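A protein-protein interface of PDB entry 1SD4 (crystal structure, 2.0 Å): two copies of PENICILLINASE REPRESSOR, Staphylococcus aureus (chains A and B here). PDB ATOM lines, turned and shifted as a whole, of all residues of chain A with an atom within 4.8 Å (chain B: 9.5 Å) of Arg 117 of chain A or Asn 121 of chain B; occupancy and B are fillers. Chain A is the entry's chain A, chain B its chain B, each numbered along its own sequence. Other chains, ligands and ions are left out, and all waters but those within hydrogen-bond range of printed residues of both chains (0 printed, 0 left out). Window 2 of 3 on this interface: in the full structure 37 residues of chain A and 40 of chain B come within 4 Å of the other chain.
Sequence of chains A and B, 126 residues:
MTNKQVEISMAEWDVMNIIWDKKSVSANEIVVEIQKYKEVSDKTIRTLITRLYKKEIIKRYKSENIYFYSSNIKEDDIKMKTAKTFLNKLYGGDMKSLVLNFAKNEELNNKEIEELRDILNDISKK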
ATOM      1  N   ILE A 113       9.396  24.907 -32.111  1.00  0.00           N
ATOM      2  CA  ILE A 113      10.250  24.334 -31.070  1.00  0.00           C
ATOM      3  C   ILE A 113      10.515  25.318 -29.928  1.00  0.00           C
ATOM      4  O   ILE A 113      10.525  24.953 -28.739  1.00  0.00           O
ATOM      5  CB  ILE A 113      11.580  23.812 -31.687  1.00  0.00           C
ATOM      6  CG1 ILE A 113      11.320  22.494 -32.429  1.00  0.00           C
ATOM      7  CG2 ILE A 113      12.674  23.587 -30.587  1.00  0.00           C
ATOM      8  CD1 ILE A 113      12.527  21.933 -33.147  1.00  0.00           C
ATOM      9  N   GLU A 114      10.694  26.578 -30.295  1.00  0.00           N
ATOM     10  CA  GLU A 114      10.906  27.629 -29.312  1.00  0.00           C
ATOM     11  C   GLU A 114       9.643  27.966 -28.564  1.00  0.00           C
ATOM     12  O   GLU A 114       9.713  28.116 -27.346  1.00  0.00           O
ATOM     13  CB  GLU A 114      11.489  28.889 -29.961  1.00  0.00           C
ATOM     14  CG  GLU A 114      12.837  28.626 -30.618  1.00  0.00           C
ATOM     15  CD  GLU A 114      13.398  29.847 -31.327  1.00  0.00           C
ATOM     16  OE1 GLU A 114      13.161  30.974 -30.830  1.00  0.00           O
ATOM     17  OE2 GLU A 114      14.083  29.664 -32.369  1.00  0.00           O
ATOM     18  N   GLU A 115       8.512  28.116 -29.283  1.00  0.00           N
ATOM     19  CA  GLU A 115       7.227  28.364 -28.645  1.00  0.00           C
ATOM     20  C   GLU A 115       6.935  27.254 -27.632  1.00  0.00           C
ATOM     21  O   GLU A 115       6.495  27.520 -26.523  1.00  0.00           O
ATOM     22  CB  GLU A 115       6.081  28.444 -29.667  1.00  0.00           C
ATOM     23  CG  GLU A 115       4.709  28.665 -29.000  1.00  0.00           C
ATOM     24  CD  GLU A 115       3.511  28.476 -29.919  1.00  0.00           C
ATOM     25  OE1 GLU A 115       3.534  27.586 -30.803  1.00  0.00           O
ATOM     26  OE2 GLU A 115       2.510  29.212 -29.732  1.00  0.00           O
ATOM     27  N   LEU A 116       7.204  26.014 -28.013  1.00  0.00           N
ATOM     28  CA  LEU A 116       6.927  24.883 -27.125  1.00  0.00           C
ATOM     29  C   LEU A 116       7.878  24.906 -25.936  1.00  0.00           C
ATOM     30  O   LEU A 116       7.475  24.670 -24.811  1.00  0.00           O
ATOM     31  CB  LEU A 116       7.009  23.531 -27.873  1.00  0.00           C
ATOM     32  CG  LEU A 116       6.607  22.273 -27.089  1.00  0.00           C
ATOM     33  CD1 LEU A 116       5.183  22.321 -26.541  1.00  0.00           C
ATOM     34  CD2 LEU A 116       6.854  20.996 -27.938  1.00  0.00           C
ATOM     35  N   ARG A 117       9.140  25.224 -26.205  1.00  0.00           N
ATOM     36  CA  ARG A 117      10.108  25.330 -25.138  1.00  0.00           C
ATOM     37  C   ARG A 117       9.638  26.395 -24.137  1.00  0.00           C
ATOM     38  O   ARG A 117       9.620  26.131 -22.931  1.00  0.00           O
ATOM     39  CB  ARG A 117      11.493  25.678 -25.688  1.00  0.00           C
ATOM     40  CG  ARG A 117      12.591  25.798 -24.626  1.00  0.00           C
ATOM     41  CD  ARG A 117      13.712  26.743 -25.044  1.00  0.00           C
ATOM     42  NE  ARG A 117      13.200  28.014 -25.586  1.00  0.00           N
ATOM     43  CZ  ARG A 117      13.877  28.775 -26.436  1.00  0.00           C
ATOM     44  NH1 ARG A 117      15.092  28.398 -26.830  1.00  0.00           N
ATOM     45  NH2 ARG A 117      13.350  29.916 -26.887  1.00  0.00           N
ATOM     46  N   ASP A 118       9.252  27.569 -24.645  1.00  0.00           N
ATOM     47  CA  ASP A 118       8.712  28.652 -23.816  1.00  0.00           C
ATOM     48  C   ASP A 118       7.519  28.214 -22.974  1.00  0.00           C
ATOM     49  O   ASP A 118       7.478  28.498 -21.777  1.00  0.00           O
ATOM     50  CB  ASP A 118       8.307  29.844 -24.678  1.00  0.00           C
ATOM     51  CG  ASP A 118       9.511  30.521 -25.359  1.00  0.00           C
ATOM     52  OD1 ASP A 118      10.676  30.164 -25.039  1.00  0.00           O
ATOM     53  OD2 ASP A 118       9.370  31.425 -26.220  1.00  0.00           O
ATOM     54  N   ILE A 119       6.590  27.482 -23.589  1.00  0.00           N
ATOM     55  CA  ILE A 119       5.425  26.984 -22.857  1.00  0.00           C
ATOM     56  C   ILE A 119       5.881  26.082 -21.696  1.00  0.00           C
ATOM     57  O   ILE A 119       5.395  26.195 -20.562  1.00  0.00           O
ATOM     58  CB  ILE A 119       4.484  26.186 -23.765  1.00  0.00           C
ATOM     59  CG1 ILE A 119       3.884  27.072 -24.862  1.00  0.00           C
ATOM     60  CG2 ILE A 119       3.390  25.507 -22.920  1.00  0.00           C
ATOM     61  CD1 ILE A 119       2.839  28.037 -24.367  1.00  0.00           C
ATOM     62  N   LEU A 120       6.819  25.191 -21.976  1.00  0.00           N
ATOM     63  CA  LEU A 120       7.261  24.260 -20.945  1.00  0.00           C
ATOM     64  C   LEU A 120       7.988  24.968 -19.825  1.00  0.00           C
ATOM     65  O   LEU A 120       7.829  24.617 -18.660  1.00  0.00           O
ATOM     66  CB  LEU A 120       8.110  23.136 -21.554  1.00  0.00           C
ATOM     67  CG  LEU A 120       7.250  22.147 -22.368  1.00  0.00           C
ATOM     68  CD1 LEU A 120       8.106  21.436 -23.430  1.00  0.00           C
ATOM     69  CD2 LEU A 120       6.632  21.137 -21.409  1.00  0.00           C
ATOM     70  N   ASN A 121       8.772  25.971 -20.183  1.00  0.00           N
ATOM     71  CA  ASN A 121       9.394  26.821 -19.188  1.00  0.00           C
ATOM     72  C   ASN A 121       8.329  27.473 -18.302  1.00  0.00           C
ATOM     73  O   ASN A 121       8.422  27.438 -17.092  1.00  0.00           O
ATOM     74  CB  ASN A 121      10.279  27.878 -19.847  1.00  0.00           C
ATOM     75  CG  ASN A 121      11.276  28.480 -18.860  1.00  0.00           C
ATOM     76  OD1 ASN A 121      11.831  27.769 -18.033  1.00  0.00           O
ATOM     77  ND2 ASN A 121      11.469  29.792 -18.919  1.00  0.00           N
ATOM     78  N   MET B  95       1.172  20.670 -31.227  1.00  0.00           N
ATOM     79  CA  MET B  95       1.922  19.935 -30.187  1.00  0.00           C
ATOM     80  C   MET B  95       1.798  20.598 -28.823  1.00  0.00           C
ATOM     81  O   MET B  95       1.790  19.931 -27.778  1.00  0.00           O
ATOM     82  CB  MET B  95       3.392  19.802 -30.593  1.00  0.00           C
ATOM     83  CG  MET B  95       4.238  18.904 -29.703  1.00  0.00           C
ATOM     84  SD  MET B  95       3.667  17.037 -29.720  1.00  0.00           S
ATOM     85  CE  MET B  95       4.359  16.643 -31.512  1.00  0.00           C
ATOM     86  N   LYS B  96       1.676  21.921 -28.811  1.00  0.00           N
ATOM     87  CA  LYS B  96       1.602  22.636 -27.527  1.00  0.00           C
ATOM     88  C   LYS B  96       0.298  22.289 -26.813  1.00  0.00           C
ATOM     89  O   LYS B  96       0.228  22.284 -25.580  1.00  0.00           O
ATOM     90  CB  LYS B  96       1.721  24.168 -27.743  1.00  0.00           C
ATOM     91  CG  LYS B  96       0.373  24.869 -27.980  1.00  0.00           C
ATOM     92  CD  LYS B  96       0.537  26.391 -28.248  1.00  0.00           C
ATOM     93  CE  LYS B  96       0.943  26.663 -29.701  1.00  0.00           C
ATOM     94  NZ  LYS B  96       0.281  27.856 -30.262  1.00  0.00           N
ATOM     95  N   VAL B  99       0.758  18.718 -25.259  1.00  0.00           N
ATOM     96  CA  VAL B  99       1.528  18.858 -24.025  1.00  0.00           C
ATOM     97  C   VAL B  99       0.727  19.503 -22.868  1.00  0.00           C
ATOM     98  O   VAL B  99       0.799  19.026 -21.730  1.00  0.00           O
ATOM     99  CB  VAL B  99       2.839  19.625 -24.270  1.00  0.00           C
ATOM    100  CG1 VAL B  99       3.658  19.710 -22.994  1.00  0.00           C
ATOM    101  CG2 VAL B  99       3.651  18.867 -25.319  1.00  0.00           C
ATOM    102  N   ILE B 113       8.501  17.528 -17.464  1.00  0.00           N
ATOM    103  CA  ILE B 113       8.299  18.847 -18.090  1.00  0.00           C
ATOM    104  C   ILE B 113       9.636  19.579 -18.221  1.00  0.00           C
ATOM    105  O   ILE B 113       9.930  20.202 -19.246  1.00  0.00           O
ATOM    106  CB  ILE B 113       7.304  19.740 -17.291  1.00  0.00           C
ATOM    107  CG1 ILE B 113       5.860  19.261 -17.427  1.00  0.00           C
ATOM    108  CG2 ILE B 113       7.451  21.237 -17.727  1.00  0.00           C
ATOM    109  CD1 ILE B 113       4.894  19.868 -16.367  1.00  0.00           C
ATOM    110  N   GLU B 114      10.413  19.554 -17.144  1.00  0.00           N
ATOM    111  CA  GLU B 114      11.723  20.207 -17.126  1.00  0.00           C
ATOM    112  C   GLU B 114      12.689  19.567 -18.126  1.00  0.00           C
ATOM    113  O   GLU B 114      13.375  20.286 -18.885  1.00  0.00           O
ATOM    114  CB  GLU B 114      12.296  20.163 -15.723  1.00  0.00           C
ATOM    115  CG  GLU B 114      11.507  21.027 -14.744  1.00  0.00           C
ATOM    116  CD  GLU B 114      11.990  20.848 -13.309  1.00  0.00           C
ATOM    117  OE1 GLU B 114      13.224  20.902 -13.081  1.00  0.00           O
ATOM    118  OE2 GLU B 114      11.157  20.660 -12.401  1.00  0.00           O
ATOM    119  N   GLU B 115      12.745  18.225 -18.106  1.00  0.00           N
ATOM    120  CA  GLU B 115      13.536  17.478 -19.054  1.00  0.00           C
ATOM    121  C   GLU B 115      13.136  17.864 -20.484  1.00  0.00           C
ATOM    122  O   GLU B 115      14.009  18.239 -21.295  1.00  0.00           O
ATOM    123  CB  GLU B 115      13.358  15.963 -18.863  1.00  0.00           C
ATOM    124  CG  GLU B 115      13.957  15.158 -20.029  1.00  0.00           C
ATOM    125  CD  GLU B 115      13.847  13.656 -19.862  1.00  0.00           C
ATOM    126  OE1 GLU B 115      12.718  13.153 -19.566  1.00  0.00           O
ATOM    127  OE2 GLU B 115      14.907  12.981 -20.047  1.00  0.00           O
ATOM    128  N   LEU B 116      11.842  17.773 -20.795  1.00  0.00           N
ATOM    129  CA  LEU B 116      11.407  18.131 -22.126  1.00  0.00           C
ATOM    130  C   LEU B 116      11.801  19.570 -22.494  1.00  0.00           C
ATOM    131  O   LEU B 116      12.243  19.857 -23.621  1.00  0.00           O
ATOM    132  CB  LEU B 116       9.912  17.940 -22.271  1.00  0.00           C
ATOM    133  CG  LEU B 116       9.480  17.925 -23.731  1.00  0.00           C
ATOM    134  CD1 LEU B 116      10.334  16.927 -24.515  1.00  0.00           C
ATOM    135  CD2 LEU B 116       8.029  17.562 -23.796  1.00  0.00           C
ATOM    136  N   ARG B 117      11.613  20.482 -21.558  1.00  0.00           N
ATOM    137  CA  ARG B 117      12.019  21.845 -21.800  1.00  0.00           C
ATOM    138  C   ARG B 117      13.511  21.854 -22.241  1.00  0.00           C
ATOM    139  O   ARG B 117      13.883  22.562 -23.182  1.00  0.00           O
ATOM    140  CB  ARG B 117      11.833  22.685 -20.534  1.00  0.00           C
ATOM    141  CG  ARG B 117      12.355  24.121 -20.709  1.00  0.00           C
ATOM    142  CD  ARG B 117      12.799  24.829 -19.440  1.00  0.00           C
ATOM    143  NE  ARG B 117      13.474  23.947 -18.479  1.00  0.00           N
ATOM    144  CZ  ARG B 117      13.455  24.120 -17.148  1.00  0.00           C
ATOM    145  NH1 ARG B 117      12.813  25.139 -16.599  1.00  0.00           N
ATOM    146  NH2 ARG B 117      14.089  23.270 -16.363  1.00  0.00           N
ATOM    147  N   ASP B 118      14.352  21.064 -21.558  1.00  0.00           N
ATOM    148  CA  ASP B 118      15.792  20.960 -21.905  1.00  0.00           C
ATOM    149  C   ASP B 118      16.055  20.366 -23.301  1.00  0.00           C
ATOM    150  O   ASP B 118      16.880  20.881 -24.084  1.00  0.00           O
ATOM    151  CB  ASP B 118      16.543  20.176 -20.838  1.00  0.00           C
ATOM    152  CG  ASP B 118      16.507  20.861 -19.464  1.00  0.00           C
ATOM    153  OD1 ASP B 118      16.297  22.077 -19.383  1.00  0.00           O
ATOM    154  OD2 ASP B 118      16.664  20.247 -18.401  1.00  0.00           O
ATOM    155  N   ILE B 119      15.332  19.314 -23.629  1.00  0.00           N
ATOM    156  CA  ILE B 119      15.485  18.662 -24.926  1.00  0.00           C
ATOM    157  C   ILE B 119      15.227  19.715 -26.038  1.00  0.00           C
ATOM    158  O   ILE B 119      16.052  19.911 -26.930  1.00  0.00           O
ATOM    159  CB  ILE B 119      14.529  17.449 -24.986  1.00  0.00           C
ATOM    160  CG1 ILE B 119      15.117  16.313 -24.130  1.00  0.00           C
ATOM    161  CG2 ILE B 119      14.289  16.984 -26.422  1.00  0.00           C
ATOM    162  CD1 ILE B 119      14.094  15.197 -23.771  1.00  0.00           C
ATOM    163  N   LEU B 120      14.119  20.431 -25.920  1.00  0.00           N
ATOM    164  CA  LEU B 120      13.710  21.419 -26.901  1.00  0.00           C
ATOM    165  C   LEU B 120      14.639  22.626 -26.935  1.00  0.00           C
ATOM    166  O   LEU B 120      14.949  23.166 -28.006  1.00  0.00           O
ATOM    167  CB  LEU B 120      12.298  21.883 -26.571  1.00  0.00           C
ATOM    168  CG  LEU B 120      11.224  20.838 -26.847  1.00  0.00           C
ATOM    169  CD1 LEU B 120       9.931  21.327 -26.268  1.00  0.00           C
ATOM    170  CD2 LEU B 120      11.105  20.558 -28.356  1.00  0.00           C
ATOM    171  N   ASN B 121      15.051  23.067 -25.757  1.00  0.00           N
ATOM    172  CA  ASN B 121      16.087  24.085 -25.668  1.00  0.00           C
ATOM    173  C   ASN B 121      17.324  23.664 -26.479  1.00  0.00           C
ATOM    174  O   ASN B 121      17.843  24.435 -27.283  1.00  0.00           O
ATOM    175  CB  ASN B 121      16.458  24.307 -24.199  1.00  0.00           C
ATOM    176  CG  ASN B 121      17.346  25.488 -24.004  1.00  0.00           C
ATOM    177  OD1 ASN B 121      16.915  26.623 -24.177  1.00  0.00           O
ATOM    178  ND2 ASN B 121      18.600  25.244 -23.648  1.00  0.00           N
ATOM    179  N   ASP B 122      17.763  22.418 -26.271  1.00  0.00           N
ATOM    180  CA  ASP B 122      18.953  21.871 -26.916  1.00  0.00           C
ATOM    181  C   ASP B 122      18.799  21.826 -28.427  1.00  0.00           C
ATOM    182  O   ASP B 122      19.704  22.249 -29.138  1.00  0.00           O
ATOM    183  CB  ASP B 122      19.265  20.460 -26.373  1.00  0.00           C
ATOM    184  CG  ASP B 122      20.416  19.775 -27.109  1.00  0.00           C
ATOM    185  OD1 ASP B 122      21.517  20.352 -27.175  1.00  0.00           O
ATOM    186  OD2 ASP B 122      20.329  18.640 -27.629  1.00  0.00           O
ATOM    187  N   ILE B 123      17.659  21.327 -28.897  1.00  0.00           N
ATOM    188  CA  ILE B 123      17.347  21.189 -30.318  1.00  0.00           C
ATOM    189  C   ILE B 123      17.407  22.523 -31.061  1.00  0.00           C
ATOM    190  O   ILE B 123      17.752  22.588 -32.244  1.00  0.00           O
ATOM    191  CB  ILE B 123      15.937  20.554 -30.485  1.00  0.00           C
ATOM    192  CG1 ILE B 123      15.966  19.095 -30.047  1.00  0.00           C
ATOM    193  CG2 ILE B 123      15.457  20.653 -31.918  1.00  0.00           C
ATOM    194  CD1 ILE B 123      14.944  18.224 -30.708  1.00  0.00           C
ATOM    195  N   SER B 124      17.065  23.584 -30.348  1.00  0.00           N
ATOM    196  CA  SER B 124      16.899  24.877 -30.957  1.00  0.00           C
ATOM    197  C   SER B 124      18.178  25.677 -30.777  1.00  0.00           C
ATOM    198  O   SER B 124      19.268  25.122 -30.543  1.00  0.00           O
ATOM    199  CB  SER B 124      15.711  25.607 -30.327  1.00  0.00           C
ATOM    200  OG  SER B 124      16.026  26.107 -29.038  1.00  0.00           O
ATOM    201  N   LYS B 125      18.019  26.985 -30.902  1.00  0.00           N
ATOM    202  CA  LYS B 125      19.027  27.938 -30.503  1.00  0.00           C
ATOM    203  C   LYS B 125      18.883  28.172 -28.984  1.00  0.00           C
ATOM    204  O   LYS B 125      19.263  27.316 -28.158  1.00  0.00           O
ATOM    205  CB  LYS B 125      18.811  29.238 -31.295  1.00  0.00           C
ATOM    206  CG  LYS B 125      19.821  29.471 -32.420  1.00  0.00           C
ATOM    207  CD  LYS B 125      19.725  30.948 -32.855  1.00  0.00           C
ATOM    208  CE  LYS B 125      20.310  31.097 -34.267  1.00  0.00           C
ATOM    209  NZ  LYS B 125      19.480  32.064 -35.035  1.00  0.00           N
ATOM    210  N   LYS B 126      18.309  29.334 -28.656  1.00  0.00           N
ATOM    211  CA  LYS B 126      18.049  29.817 -27.299  1.00  0.00           C
ATOM    212  C   LYS B 126      16.938  30.883 -27.420  1.00  0.00           C
ATOM    213  O   LYS B 126      17.116  32.021 -26.931  1.00  0.00           O
ATOM    214  CB  LYS B 126      19.327  30.411 -26.644  1.00  0.00           C
ATOM    215  CG  LYS B 126      20.321  29.361 -26.019  1.00  0.00           C
ATOM    216  CD  LYS B 126      21.535  29.993 -25.281  1.00  0.00           C
ATOM    217  CE  LYS B 126      22.167  28.935 -24.365  1.00  0.00           C
ATOM    218  NZ  LYS B 126      23.489  29.352 -23.759  1.00  0.00           N
ATOM    219  OXT LYS B 126      15.888  30.554 -28.011  1.00  0.00           O
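NZ of Lys 96 of chain B is in salt-bridge range of OE2 of Glu 115 of chain A (2.7 Å). OG of Ser 124 of chain B is in hydrogen-bond range of NH1 of Arg 117 of chain A (3.3 Å). NH1 of Arg 117 of chain A lies within salt-bridge range of OXT of Lys 126 of chain B, 2.6 Å away. The guanidinium group of Arg 117 of chain B sits at hydrogen-bond distance from the side-chain amide oxygen of Asn 121 of chain A.
NH2 of Arg 117 of chain A is in salt-bridge range of OD1 of Asp 118 of chain A, at 3.3 Å. The guanidinium group of Arg 117 of chain B is in salt-bridge range of the side-chain carboxylate of Asp 118 of chain B, at 3.5 Å. The backbone carbonyl oxygen (O) of Leu 120 of chain B lies within hydrogen-bond range of the side-chain hydroxyl (OG) of Ser 124 of chain B, 3.3 Å away. O of Asn 121 of chain B lies within hydrogen-bond range of OG of Ser 124 of chain B, at 3.0 Å.
Leu 120 of chain B touches Ile 113 of chain A. Ile 113 of chain A touches Ser 124 of chain B. OE1 of Glu 114 of chain A touches OXT of Lys 126 of chain B, 3.9 Å away. Met 95 of chain B touches Leu 116 of chain A. CD1 of Leu 116 of chain A touches CA of Lys 96 of chain B, 3.7 Å away. Leu 116 of chain A touches Val 99 of chain B (CD1 to CG2, 3.97 Å). Arg 117 of chain A touches Arg 117 of chain B. Arg 117 of chain A touches Leu 120 of chain B (N to CD1, 3.98 Å). Leu 120 of chain A touches Val 99 of chain B (CD2 to CG1, 3.7 Å). Leu 116 of chain B touches Leu 120 of chain A.
Arg 117 of chain A touches just these residues of chain B: Arg 117, Leu 120, Asn 121, Ser 124 and Lys 126. Asn 121 of chain B touches one residue of chain A. No residue of chain B comes within 4 Å of Asp 118 of chain A. Of the printed residues of chain A, Val 99 of chain B touches Leu 116 (3.97 Å) and Leu 120 (3.7 Å). Of the printed residues of chain A, Met 95 of chain B touches Leu 116. Of the printed residues of chain A, Lys 126 of chain B touches Glu 114 (3.9 Å) and Arg 117 (2.6 Å). Of the printed residues of chain A, Leu 120 of chain B touches Ile 113, Leu 116, Arg 117 and Leu 120. Of the printed residues of chain B, Ile 113 of chain A touches Leu 120, Ile 123 and Ser 124. The nearest printed residue of chain A that does not touch Asn 121 of chain B is Ile 113 of chain A (5.4 Å). The nearest printed residue of chain B that does not touch Asn 121 of chain A is Ile 113 of chain B (5.5 Å).
Of the 9 printed residues of chain A, 7 touch a printed residue of chain B. Printed residues of chain A that touch a printed residue of chain B: Ile 113, Glu 114, Glu 115, Leu 116, Arg 117, Leu 120 and Asn 121. Hydrophobic or aromatic side chains of chain A within 4 Å of the printed part of chain B: Ile 113, Leu 116 and Leu 120. Among the printed residues, Asp or Glu carboxylates within 4 Å of a Lys or Arg side-chain nitrogen of the other chain: Glu 115 of chain A with Lys 96 of chain B (2.7 Å).
Leu 116 of chain A touches Leu 120 of chain B, and with the chains exchanged Leu 120 of chain A touches Leu 116 of chain B. Arg 117 of chain B touches its own counterpart, Arg 117 of chain A. Arg 117 of chain A touches Leu 120 of chain B, and with the chains exchanged Leu 120 of chain A touches Arg 117 of chain B. Arg 117 of chain A touches Asn 121 of chain B, and with the chains exchanged Asn 121 of chain A touches Arg 117 of chain B.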
